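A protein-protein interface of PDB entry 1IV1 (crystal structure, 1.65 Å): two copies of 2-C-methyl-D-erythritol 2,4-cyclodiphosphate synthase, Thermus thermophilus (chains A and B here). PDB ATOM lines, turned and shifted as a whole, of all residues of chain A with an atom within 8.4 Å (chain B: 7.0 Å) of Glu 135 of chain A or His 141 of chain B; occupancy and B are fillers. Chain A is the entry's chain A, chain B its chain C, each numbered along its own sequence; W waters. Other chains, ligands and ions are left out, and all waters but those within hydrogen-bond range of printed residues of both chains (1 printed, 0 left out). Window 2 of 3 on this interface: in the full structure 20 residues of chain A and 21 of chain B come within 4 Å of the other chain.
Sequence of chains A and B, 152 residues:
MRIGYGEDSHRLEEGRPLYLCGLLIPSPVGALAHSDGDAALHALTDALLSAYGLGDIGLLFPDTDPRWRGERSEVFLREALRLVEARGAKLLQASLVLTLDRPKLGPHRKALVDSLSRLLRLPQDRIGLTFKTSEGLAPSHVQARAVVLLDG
The backbone carbonyl oxygen (O) of His 10 of chain B is in hydrogen-bond range of the backbone NH (N) of Val 142 of chain B (2.9 Å).
OG of Ser 134 of chain A is in hydrogen-bond range of N of Ala 138 of chain A, at 2.8 Å.
The backbone NH of Arg 11 of chain B lies within hydrogen-bond range of a ring nitrogen (ND1) of His 141 of chain B (3.5 Å).
The side-chain hydroxyl (OG) of Ser 134 of chain A lies within hydrogen-bond range of the backbone NH (N) of Leu 137 of chain A (3.3 Å).
The side-chain hydroxyl (OG1) of Thr 133 of chain A sits close to the backbone NH (N) of Glu 135 of chain A (3.5 Å).
The backbone NH (N) of Leu 100 of chain A sits at hydrogen-bond distance from the backbone carbonyl oxygen (O) of Lys 132 of chain A (3.1 Å).
Of chain A, only Ser 134, Glu 135 and Leu 137 come within 4 Å of His 141 of chain B.
Of the printed residues of chain A, Arg 11 of chain B touches Glu 135.
Of the printed residues of chain A, Ser 9 of chain B touches Ser 134 (3.6 Å) and Glu 135 (3.6 Å).
Of the printed residues of chain A, His 10 of chain B touches Glu 135.
Of the printed residues of chain A, Ala 138 of chain B touches Leu 137.
Thr 99 of chain B touches none of the printed residues of chain A.
Leu 100 of chain A touches none of the printed residues of chain B.
The nearest printed residue of chain A that does not touch His 10 of chain B is Lys 132 of chain A (5.6 Å).
OG of Ser 9 of chain B touches O of Ser 134 of chain A, at 3.6 Å.
Ser 134 of chain A touches His 141 of chain B.
CD of Glu 135 of chain A touches O of Ser 9 of chain B, at 3.6 Å.
Ala 138 of chain B touches Leu 137 of chain A.
CB of Leu 137 of chain A touches NE2 of His 141 of chain B (3.5 Å).
Water W1 lies within hydrogen-bond range of OD1 of Asp 8 of chain B, O of Ser 9 of chain B and NZ of Lys 132 of chain A.
The backbone NH (N) of Arg 11 of chain B is in hydrogen-bond range of the side-chain carboxylate (OE2) of Glu 135 of chain A, at 2.8 Å.
NZ of Lys 132 of chain A lies within salt-bridge range of OD1 of Asp 8 of chain B, 2.5 Å away.
The side-chain carboxylate (OE1) of Glu 135 of chain A sits at hydrogen-bond distance from a ring nitrogen (ND1) of His 10 of chain B, 2.5 Å away.
The backbone carbonyl oxygen (O) of Glu 135 of chain A lies close to a ring nitrogen (NE2) of His 141 of chain B (3.5 Å).
Of the 12 printed residues of chain A, 4 touch a printed residue of chain B.
Along chain A the printed residues that touch a printed residue of chain B span positions 132 to 137.
Hydrophobic or aromatic side chains of chain B that line the printed part of chain A: His 10, Ala 138 and His 141.
Along chain B the printed residues that touch a printed residue of chain A span positions 8 to 141.
Among the printed residues, 9 pairs touch across the chains.
Among the printed residues, Asp or Glu carboxylates within 4 Å of a Lys or Arg side-chain nitrogen of the other chain: Lys 132 of chain A with Asp 8 of chain B (2.5 Å).
Positions printed for both chains: 99, 100, 101, 134, 138, 139 and 143.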
ATOM      1  N   THR A  99       4.822  14.331   8.103  1.00  0.00           N
ATOM      2  CA  THR A  99       3.770  14.028   9.067  1.00  0.00           C
ATOM      3  C   THR A  99       2.707  15.118   9.029  1.00  0.00           C
ATOM      4  O   THR A  99       2.944  16.301   9.290  1.00  0.00           O
ATOM      5  CB  THR A  99       4.396  13.863  10.463  1.00  0.00           C
ATOM      6  OG1 THR A  99       5.391  12.831  10.417  1.00  0.00           O
ATOM      7  CG2 THR A  99       3.379  13.396  11.496  1.00  0.00           C
ATOM      8  N   LEU A 100       1.492  14.734   8.669  1.00  0.00           N
ATOM      9  CA  LEU A 100       0.371  15.656   8.566  1.00  0.00           C
ATOM     10  C   LEU A 100      -0.919  14.849   8.503  1.00  0.00           C
ATOM     11  O   LEU A 100      -1.052  13.870   7.777  1.00  0.00           O
ATOM     12  CB  LEU A 100       0.531  16.576   7.359  1.00  0.00           C
ATOM     13  CG  LEU A 100       0.094  16.048   5.991  1.00  0.00           C
ATOM     14  CD1 LEU A 100       0.174  17.153   4.949  1.00  0.00           C
ATOM     15  CD2 LEU A 100       0.924  14.847   5.568  1.00  0.00           C
ATOM     16  N   ASP A 101      -1.894  15.268   9.304  1.00  0.00           N
ATOM     17  CA  ASP A 101      -3.127  14.492   9.420  1.00  0.00           C
ATOM     18  C   ASP A 101      -4.007  14.635   8.193  1.00  0.00           C
ATOM     19  O   ASP A 101      -4.847  13.764   7.947  1.00  0.00           O
ATOM     20  CB  ASP A 101      -3.832  14.895  10.725  1.00  0.00           C
ATOM     21  CG  ASP A 101      -3.074  14.411  11.950  1.00  0.00           C
ATOM     22  OD1 ASP A 101      -1.901  13.974  11.866  1.00  0.00           O
ATOM     23  OD2 ASP A 101      -3.657  14.447  13.064  1.00  0.00           O
ATOM     24  N   LYS A 132       3.238  10.042   6.913  1.00  0.00           N
ATOM     25  CA  LYS A 132       2.585   9.571   8.136  1.00  0.00           C
ATOM     26  C   LYS A 132       1.487  10.509   8.600  1.00  0.00           C
ATOM     27  O   LYS A 132       1.486  11.687   8.242  1.00  0.00           O
ATOM     28  CB  LYS A 132       3.612   9.471   9.271  1.00  0.00           C
ATOM     29  CG  LYS A 132       4.841   8.638   8.977  1.00  0.00           C
ATOM     30  CD  LYS A 132       4.482   7.228   8.551  1.00  0.00           C
ATOM     31  CE  LYS A 132       4.748   6.190   9.618  1.00  0.00           C
ATOM     32  NZ  LYS A 132       3.473   5.728  10.259  1.00  0.00           N
ATOM     33  N   THR A 133       0.562  10.033   9.440  1.00  0.00           N
ATOM     34  CA  THR A 133      -0.298  10.970  10.143  1.00  0.00           C
ATOM     35  C   THR A 133       0.197  11.109  11.588  1.00  0.00           C
ATOM     36  O   THR A 133       0.935  10.225  12.033  1.00  0.00           O
ATOM     37  CB  THR A 133      -1.777  10.557  10.217  1.00  0.00           C
ATOM     38  OG1 THR A 133      -1.857   9.385  11.042  1.00  0.00           O
ATOM     39  CG2 THR A 133      -2.320  10.234   8.840  1.00  0.00           C
ATOM     40  N   SER A 134      -0.212  12.176  12.284  1.00  0.00           N
ATOM     41  CA  SER A 134       0.196  12.288  13.686  1.00  0.00           C
ATOM     42  C   SER A 134      -0.790  11.617  14.650  1.00  0.00           C
ATOM     43  O   SER A 134      -0.556  11.742  15.857  1.00  0.00           O
ATOM     44  CB  SER A 134       0.388  13.742  14.122  1.00  0.00           C
ATOM     45  OG  SER A 134      -0.818  14.477  14.168  1.00  0.00           O
ATOM     46  N   GLU A 135      -1.814  10.958  14.158  1.00  0.00           N
ATOM     47  CA  GLU A 135      -2.823  10.296  14.990  1.00  0.00           C
ATOM     48  C   GLU A 135      -3.302  11.267  16.062  1.00  0.00           C
ATOM     49  O   GLU A 135      -3.402  10.918  17.230  1.00  0.00           O
ATOM     50  CB  GLU A 135      -2.281   9.010  15.606  1.00  0.00           C
ATOM     51  CG  GLU A 135      -2.083   7.903  14.580  1.00  0.00           C
ATOM     52  CD  GLU A 135      -2.126   6.501  15.144  1.00  0.00           C
ATOM     53  OE1 GLU A 135      -1.804   5.555  14.389  1.00  0.00           O
ATOM     54  OE2 GLU A 135      -2.479   6.314  16.326  1.00  0.00           O
ATOM     55  N   GLY A 136      -3.557  12.481  15.582  1.00  0.00           N
ATOM     56  CA  GLY A 136      -4.037  13.580  16.374  1.00  0.00           C
ATOM     57  C   GLY A 136      -3.043  14.203  17.321  1.00  0.00           C
ATOM     58  O   GLY A 136      -3.432  15.072  18.109  1.00  0.00           O
ATOM     59  N   LEU A 137      -1.770  13.795  17.289  1.00  0.00           N
ATOM     60  CA  LEU A 137      -0.812  14.470  18.170  1.00  0.00           C
ATOM     61  C   LEU A 137      -0.461  15.871  17.685  1.00  0.00           C
ATOM     62  O   LEU A 137      -0.004  16.719  18.462  1.00  0.00           O
ATOM     63  CB  LEU A 137       0.433  13.590  18.316  1.00  0.00           C
ATOM     64  CG  LEU A 137       1.615  14.253  19.035  1.00  0.00           C
ATOM     65  CD1 LEU A 137       1.197  14.761  20.406  1.00  0.00           C
ATOM     66  CD2 LEU A 137       2.786  13.286  19.127  1.00  0.00           C
ATOM     67  N   ALA A 138      -0.665  16.177  16.408  1.00  0.00           N
ATOM     68  CA  ALA A 138      -0.357  17.487  15.828  1.00  0.00           C
ATOM     69  C   ALA A 138      -1.253  17.708  14.619  1.00  0.00           C
ATOM     70  O   ALA A 138      -0.771  17.735  13.493  1.00  0.00           O
ATOM     71  CB  ALA A 138       1.101  17.588  15.434  1.00  0.00           C
ATOM     72  N   PRO A 139      -2.557  17.836  14.851  1.00  0.00           N
ATOM     73  CA  PRO A 139      -3.538  17.807  13.766  1.00  0.00           C
ATOM     74  C   PRO A 139      -3.608  19.096  12.952  1.00  0.00           C
ATOM     75  O   PRO A 139      -4.283  19.127  11.922  1.00  0.00           O
ATOM     76  CB  PRO A 139      -4.869  17.589  14.502  1.00  0.00           C
ATOM     77  CG  PRO A 139      -4.637  18.122  15.872  1.00  0.00           C
ATOM     78  CD  PRO A 139      -3.172  18.013  16.174  1.00  0.00           C
ATOM     79  N   GLN A 143       4.785  18.531   9.626  1.00  0.00           N
ATOM     80  CA  GLN A 143       6.141  18.339  10.117  1.00  0.00           C
ATOM     81  C   GLN A 143       6.970  17.579   9.077  1.00  0.00           C
ATOM     82  O   GLN A 143       6.399  16.722   8.403  1.00  0.00           O
ATOM     83  CB  GLN A 143       6.205  17.566  11.430  1.00  0.00           C
ATOM     84  CG  GLN A 143       5.163  17.961  12.464  1.00  0.00           C
ATOM     85  CD  GLN A 143       5.056  16.947  13.597  1.00  0.00           C
ATOM     86  OE1 GLN A 143       4.079  16.216  13.764  1.00  0.00           O
ATOM     87  NE2 GLN A 143       6.093  16.898  14.428  1.00  0.00           N
ATOM     88  N   ASP B   8       7.227   6.706  13.371  1.00  0.00           N
ATOM     89  CA  ASP B   8       5.817   6.345  13.509  1.00  0.00           C
ATOM     90  C   ASP B   8       5.383   6.789  14.900  1.00  0.00           C
ATOM     91  O   ASP B   8       6.221   6.814  15.789  1.00  0.00           O
ATOM     92  CB  ASP B   8       5.552   4.866  13.291  1.00  0.00           C
ATOM     93  CG  ASP B   8       4.054   4.590  13.261  1.00  0.00           C
ATOM     94  OD1 ASP B   8       3.324   5.447  12.714  1.00  0.00           O
ATOM     95  OD2 ASP B   8       3.633   3.549  13.793  1.00  0.00           O
ATOM     96  N   SER B   9       4.105   7.104  15.041  1.00  0.00           N
ATOM     97  CA  SER B   9       3.520   7.473  16.332  1.00  0.00           C
ATOM     98  C   SER B   9       2.084   6.971  16.354  1.00  0.00           C
ATOM     99  O   SER B   9       1.385   7.066  15.342  1.00  0.00           O
ATOM    100  CB  SER B   9       3.573   8.980  16.565  1.00  0.00           C
ATOM    101  OG  SER B   9       2.277   9.533  16.385  1.00  0.00           O
ATOM    102  N   HIS B  10       1.677   6.427  17.495  1.00  0.00           N
ATOM    103  CA  HIS B  10       0.322   5.904  17.621  1.00  0.00           C
ATOM    104  C   HIS B  10      -0.281   6.396  18.932  1.00  0.00           C
ATOM    105  O   HIS B  10       0.407   6.502  19.950  1.00  0.00           O
ATOM    106  CB  HIS B  10       0.317   4.379  17.584  1.00  0.00           C
ATOM    107  CG  HIS B  10       0.571   3.759  16.252  1.00  0.00           C
ATOM    108  ND1 HIS B  10      -0.377   3.728  15.250  1.00  0.00           N
ATOM    109  CD2 HIS B  10       1.671   3.143  15.750  1.00  0.00           C
ATOM    110  CE1 HIS B  10       0.128   3.121  14.195  1.00  0.00           C
ATOM    111  NE2 HIS B  10       1.370   2.752  14.469  1.00  0.00           N
ATOM    112  N   ARG B  11      -1.561   6.700  18.890  1.00  0.00           N
ATOM    113  CA  ARG B  11      -2.267   7.061  20.118  1.00  0.00           C
ATOM    114  C   ARG B  11      -2.308   5.905  21.109  1.00  0.00           C
ATOM    115  O   ARG B  11      -2.553   4.741  20.780  1.00  0.00           O
ATOM    116  CB  ARG B  11      -3.669   7.526  19.699  1.00  0.00           C
ATOM    117  CG  ARG B  11      -4.551   7.983  20.839  1.00  0.00           C
ATOM    118  CD  ARG B  11      -5.870   8.559  20.343  1.00  0.00           C
ATOM    119  NE  ARG B  11      -5.731   9.931  19.859  1.00  0.00           N
ATOM    120  CZ  ARG B  11      -5.425  10.955  20.644  1.00  0.00           C
ATOM    121  NH1 ARG B  11      -5.229  10.743  21.939  1.00  0.00           N
ATOM    122  NH2 ARG B  11      -5.308  12.184  20.156  1.00  0.00           N
ATOM    123  N   LEU B  12      -2.069   6.189  22.393  1.00  0.00           N
ATOM    124  CA  LEU B  12      -2.123   5.114  23.380  1.00  0.00           C
ATOM    125  C   LEU B  12      -3.494   5.112  24.045  1.00  0.00           C
ATOM    126  O   LEU B  12      -4.039   6.145  24.410  1.00  0.00           O
ATOM    127  CB  LEU B  12      -1.017   5.231  24.422  1.00  0.00           C
ATOM    128  CG  LEU B  12       0.406   5.035  23.878  1.00  0.00           C
ATOM    129  CD1 LEU B  12       1.430   5.686  24.795  1.00  0.00           C
ATOM    130  CD2 LEU B  12       0.739   3.570  23.684  1.00  0.00           C
ATOM    131  N   ALA B  31      -1.549   0.601  22.087  1.00  0.00           N
ATOM    132  CA  ALA B  31      -1.922   1.465  20.954  1.00  0.00           C
ATOM    133  C   ALA B  31      -3.377   1.220  20.597  1.00  0.00           C
ATOM    134  O   ALA B  31      -3.914   0.118  20.615  1.00  0.00           O
ATOM    135  CB  ALA B  31      -0.985   1.280  19.779  1.00  0.00           C
ATOM    136  N   LEU B  32      -4.049   2.328  20.282  1.00  0.00           N
ATOM    137  CA  LEU B  32      -5.356   2.188  19.658  1.00  0.00           C
ATOM    138  C   LEU B  32      -5.058   2.204  18.159  1.00  0.00           C
ATOM    139  O   LEU B  32      -4.793   3.270  17.608  1.00  0.00           O
ATOM    140  CB  LEU B  32      -6.319   3.274  20.072  1.00  0.00           C
ATOM    141  CG  LEU B  32      -7.157   3.898  18.954  1.00  0.00           C
ATOM    142  CD1 LEU B  32      -8.638   3.817  19.278  1.00  0.00           C
ATOM    143  CD2 LEU B  32      -6.689   5.328  18.716  1.00  0.00           C
ATOM    144  N   ALA B  33      -5.058   1.013  17.568  1.00  0.00           N
ATOM    145  CA  ALA B  33      -4.696   0.870  16.167  1.00  0.00           C
ATOM    146  C   ALA B  33      -5.432  -0.287  15.497  1.00  0.00           C
ATOM    147  O   ALA B  33      -5.876  -1.229  16.147  1.00  0.00           O
ATOM    148  CB  ALA B  33      -3.196   0.655  15.995  1.00  0.00           C
ATOM    149  N   HIS B  34      -5.520  -0.153  14.179  1.00  0.00           N
ATOM    150  CA  HIS B  34      -6.058  -1.188  13.309  1.00  0.00           C
ATOM    151  C   HIS B  34      -4.955  -2.197  12.974  1.00  0.00           C
ATOM    152  O   HIS B  34      -5.224  -3.197  12.304  1.00  0.00           O
ATOM    153  CB  HIS B  34      -6.674  -0.546  12.068  1.00  0.00           C
ATOM    154  CG  HIS B  34      -7.836   0.351  12.390  1.00  0.00           C
ATOM    155  ND1 HIS B  34      -8.201   0.673  13.676  1.00  0.00           N
ATOM    156  CD2 HIS B  34      -8.719   0.986  11.577  1.00  0.00           C
ATOM    157  CE1 HIS B  34      -9.254   1.469  13.655  1.00  0.00           C
ATOM    158  NE2 HIS B  34      -9.589   1.675  12.398  1.00  0.00           N
ATOM    159  N   SER B  35      -3.760  -1.909  13.463  1.00  0.00           N
ATOM    160  CA  SER B  35      -2.550  -2.720  13.501  1.00  0.00           C
ATOM    161  C   SER B  35      -2.243  -3.055  14.962  1.00  0.00           C
ATOM    162  O   SER B  35      -3.116  -2.837  15.816  1.00  0.00           O
ATOM    163  CB  SER B  35      -1.383  -1.995  12.834  1.00  0.00           C
ATOM    164  OG  SER B  35      -1.011  -0.820  13.537  1.00  0.00           O
ATOM    165  N   GLY B  37       0.009  -1.503  16.552  1.00  0.00           N
ATOM    166  CA  GLY B  37       0.493  -0.213  16.980  1.00  0.00           C
ATOM    167  C   GLY B  37       1.947  -0.186  17.374  1.00  0.00           C
ATOM    168  O   GLY B  37       2.340   0.713  18.112  1.00  0.00           O
ATOM    169  N   THR B  99       9.654   6.999  22.434  1.00  0.00           N
ATOM    170  CA  THR B  99       9.247   8.014  23.401  1.00  0.00           C
ATOM    171  C   THR B  99       7.823   7.777  23.881  1.00  0.00           C
ATOM    172  O   THR B  99       6.906   7.764  23.066  1.00  0.00           O
ATOM    173  CB  THR B  99       9.273   9.432  22.785  1.00  0.00           C
ATOM    174  OG1 THR B  99      10.568   9.671  22.243  1.00  0.00           O
ATOM    175  CG2 THR B  99       9.006  10.468  23.860  1.00  0.00           C
ATOM    176  N   LEU B 100       7.659   7.639  25.189  1.00  0.00           N
ATOM    177  CA  LEU B 100       6.313   7.475  25.745  1.00  0.00           C
ATOM    178  C   LEU B 100       6.388   7.738  27.250  1.00  0.00           C
ATOM    179  O   LEU B 100       7.422   7.481  27.862  1.00  0.00           O
ATOM    180  CB  LEU B 100       5.696   6.127  25.440  1.00  0.00           C
ATOM    181  CG  LEU B 100       6.211   4.864  26.112  1.00  0.00           C
ATOM    182  CD1 LEU B 100       5.507   3.630  25.560  1.00  0.00           C
ATOM    183  CD2 LEU B 100       7.712   4.737  25.940  1.00  0.00           C
ATOM    184  N   ASP B 101       5.273   8.256  27.765  1.00  0.00           N
ATOM    185  CA  ASP B 101       5.342   8.759  29.144  1.00  0.00           C
ATOM    186  C   ASP B 101       5.219   7.620  30.147  1.00  0.00           C
ATOM    187  O   ASP B 101       5.807   7.729  31.232  1.00  0.00           O
ATOM    188  CB  ASP B 101       4.310   9.880  29.324  1.00  0.00           C
ATOM    189  CG  ASP B 101       4.858  11.192  28.773  1.00  0.00           C
ATOM    190  OD1 ASP B 101       5.681  11.173  27.825  1.00  0.00           O
ATOM    191  OD2 ASP B 101       4.489  12.276  29.270  1.00  0.00           O
ATOM    192  N   ARG B 102       4.512   6.568  29.795  1.00  0.00           N
ATOM    193  CA  ARG B 102       4.314   5.332  30.535  1.00  0.00           C
ATOM    194  C   ARG B 102       4.031   4.210  29.536  1.00  0.00           C
ATOM    195  O   ARG B 102       3.529   4.550  28.445  1.00  0.00           O
ATOM    196  CB  ARG B 102       3.174   5.467  31.543  1.00  0.00           C
ATOM    197  CG  ARG B 102       1.953   6.203  31.014  1.00  0.00           C
ATOM    198  CD  ARG B 102       1.022   6.658  32.128  1.00  0.00           C
ATOM    199  NE  ARG B 102      -0.394   6.444  31.800  1.00  0.00           N
ATOM    200  CZ  ARG B 102      -1.200   5.682  32.539  1.00  0.00           C
ATOM    201  NH1 ARG B 102      -0.736   5.073  33.628  1.00  0.00           N
ATOM    202  NH2 ARG B 102      -2.476   5.497  32.234  1.00  0.00           N
ATOM    203  N   SER B 134       8.118  11.896  27.083  1.00  0.00           N
ATOM    204  CA  SER B 134       7.823  13.133  26.367  1.00  0.00           C
ATOM    205  C   SER B 134       7.815  14.326  27.320  1.00  0.00           C
ATOM    206  O   SER B 134       7.594  15.469  26.904  1.00  0.00           O
ATOM    207  CB  SER B 134       6.494  13.058  25.619  1.00  0.00           C
ATOM    208  OG  SER B 134       5.416  13.532  26.395  1.00  0.00           O
ATOM    209  N   ALA B 138       3.681  14.798  24.985  1.00  0.00           N
ATOM    210  CA  ALA B 138       2.858  13.846  24.250  1.00  0.00           C
ATOM    211  C   ALA B 138       2.436  12.655  25.101  1.00  0.00           C
ATOM    212  O   ALA B 138       2.781  11.499  24.873  1.00  0.00           O
ATOM    213  CB  ALA B 138       3.607  13.339  23.009  1.00  0.00           C
ATOM    214  N   PRO B 139       1.632  12.870  26.131  1.00  0.00           N
ATOM    215  CA  PRO B 139       1.438  11.818  27.130  1.00  0.00           C
ATOM    216  C   PRO B 139       0.432  10.760  26.708  1.00  0.00           C
ATOM    217  O   PRO B 139       0.229   9.806  27.468  1.00  0.00           O
ATOM    218  CB  PRO B 139       0.891  12.622  28.326  1.00  0.00           C
ATOM    219  CG  PRO B 139       0.116  13.728  27.685  1.00  0.00           C
ATOM    220  CD  PRO B 139       0.840  14.075  26.417  1.00  0.00           C
ATOM    221  N   SER B 140      -0.191  10.913  25.543  1.00  0.00           N
ATOM    222  CA  SER B 140      -1.153   9.934  25.046  1.00  0.00           C
ATOM    223  C   SER B 140      -0.706   9.231  23.773  1.00  0.00           C
ATOM    224  O   SER B 140      -1.492   8.628  23.037  1.00  0.00           O
ATOM    225  CB  SER B 140      -2.504  10.635  24.830  1.00  0.00           C
ATOM    226  OG  SER B 140      -2.710  11.589  25.864  1.00  0.00           O
ATOM    227  N   HIS B 141       0.591   9.293  23.486  1.00  0.00           N
ATOM    228  CA  HIS B 141       1.127   8.676  22.291  1.00  0.00           C
ATOM    229  C   HIS B 141       2.413   7.916  22.571  1.00  0.00           C
ATOM    230  O   HIS B 141       3.150   8.317  23.487  1.00  0.00           O
ATOM    231  CB  HIS B 141       1.478   9.728  21.209  1.00  0.00           C
ATOM    232  CG  HIS B 141       0.233  10.301  20.615  1.00  0.00           C
ATOM    233  ND1 HIS B 141      -0.278   9.892  19.413  1.00  0.00           N
ATOM    234  CD2 HIS B 141      -0.604  11.254  21.088  1.00  0.00           C
ATOM    235  CE1 HIS B 141      -1.378  10.567  19.143  1.00  0.00           C
ATOM    236  NE2 HIS B 141      -1.582  11.392  20.144  1.00  0.00           N
ATOM    237  N   VAL B 142       2.653   6.908  21.747  1.00  0.00           N
ATOM    238  CA  VAL B 142       4.004   6.333  21.673  1.00  0.00           C
ATOM    239  C   VAL B 142       4.661   6.866  20.396  1.00  0.00           C
ATOM    240  O   VAL B 142       3.988   6.873  19.366  1.00  0.00           O
ATOM    241  CB  VAL B 142       3.988   4.809  21.720  1.00  0.00           C
ATOM    242  CG1 VAL B 142       3.040   4.253  20.654  1.00  0.00           C
ATOM    243  CG2 VAL B 142       5.402   4.253  21.584  1.00  0.00           C
ATOM    244  N   GLN B 143       5.906   7.326  20.468  1.00  0.00           N
ATOM    245  CA  GLN B 143       6.527   7.834  19.218  1.00  0.00           C
ATOM    246  C   GLN B 143       7.783   7.037  18.928  1.00  0.00           C
ATOM    247  O   GLN B 143       8.507   6.660  19.853  1.00  0.00           O
ATOM    248  CB  GLN B 143       6.874   9.309  19.327  1.00  0.00           C
ATOM    249  CG  GLN B 143       5.845  10.212  19.999  1.00  0.00           C
ATOM    250  CD  GLN B 143       6.395  11.593  20.281  1.00  0.00           C
ATOM    251  OE1 GLN B 143       6.484  12.035  21.429  1.00  0.00           O
ATOM    252  NE2 GLN B 143       6.795  12.307  19.228  1.00  0.00           N
HETATM  253  O   HOH W   1       0.952   6.574  12.276  1.00  0.00           O
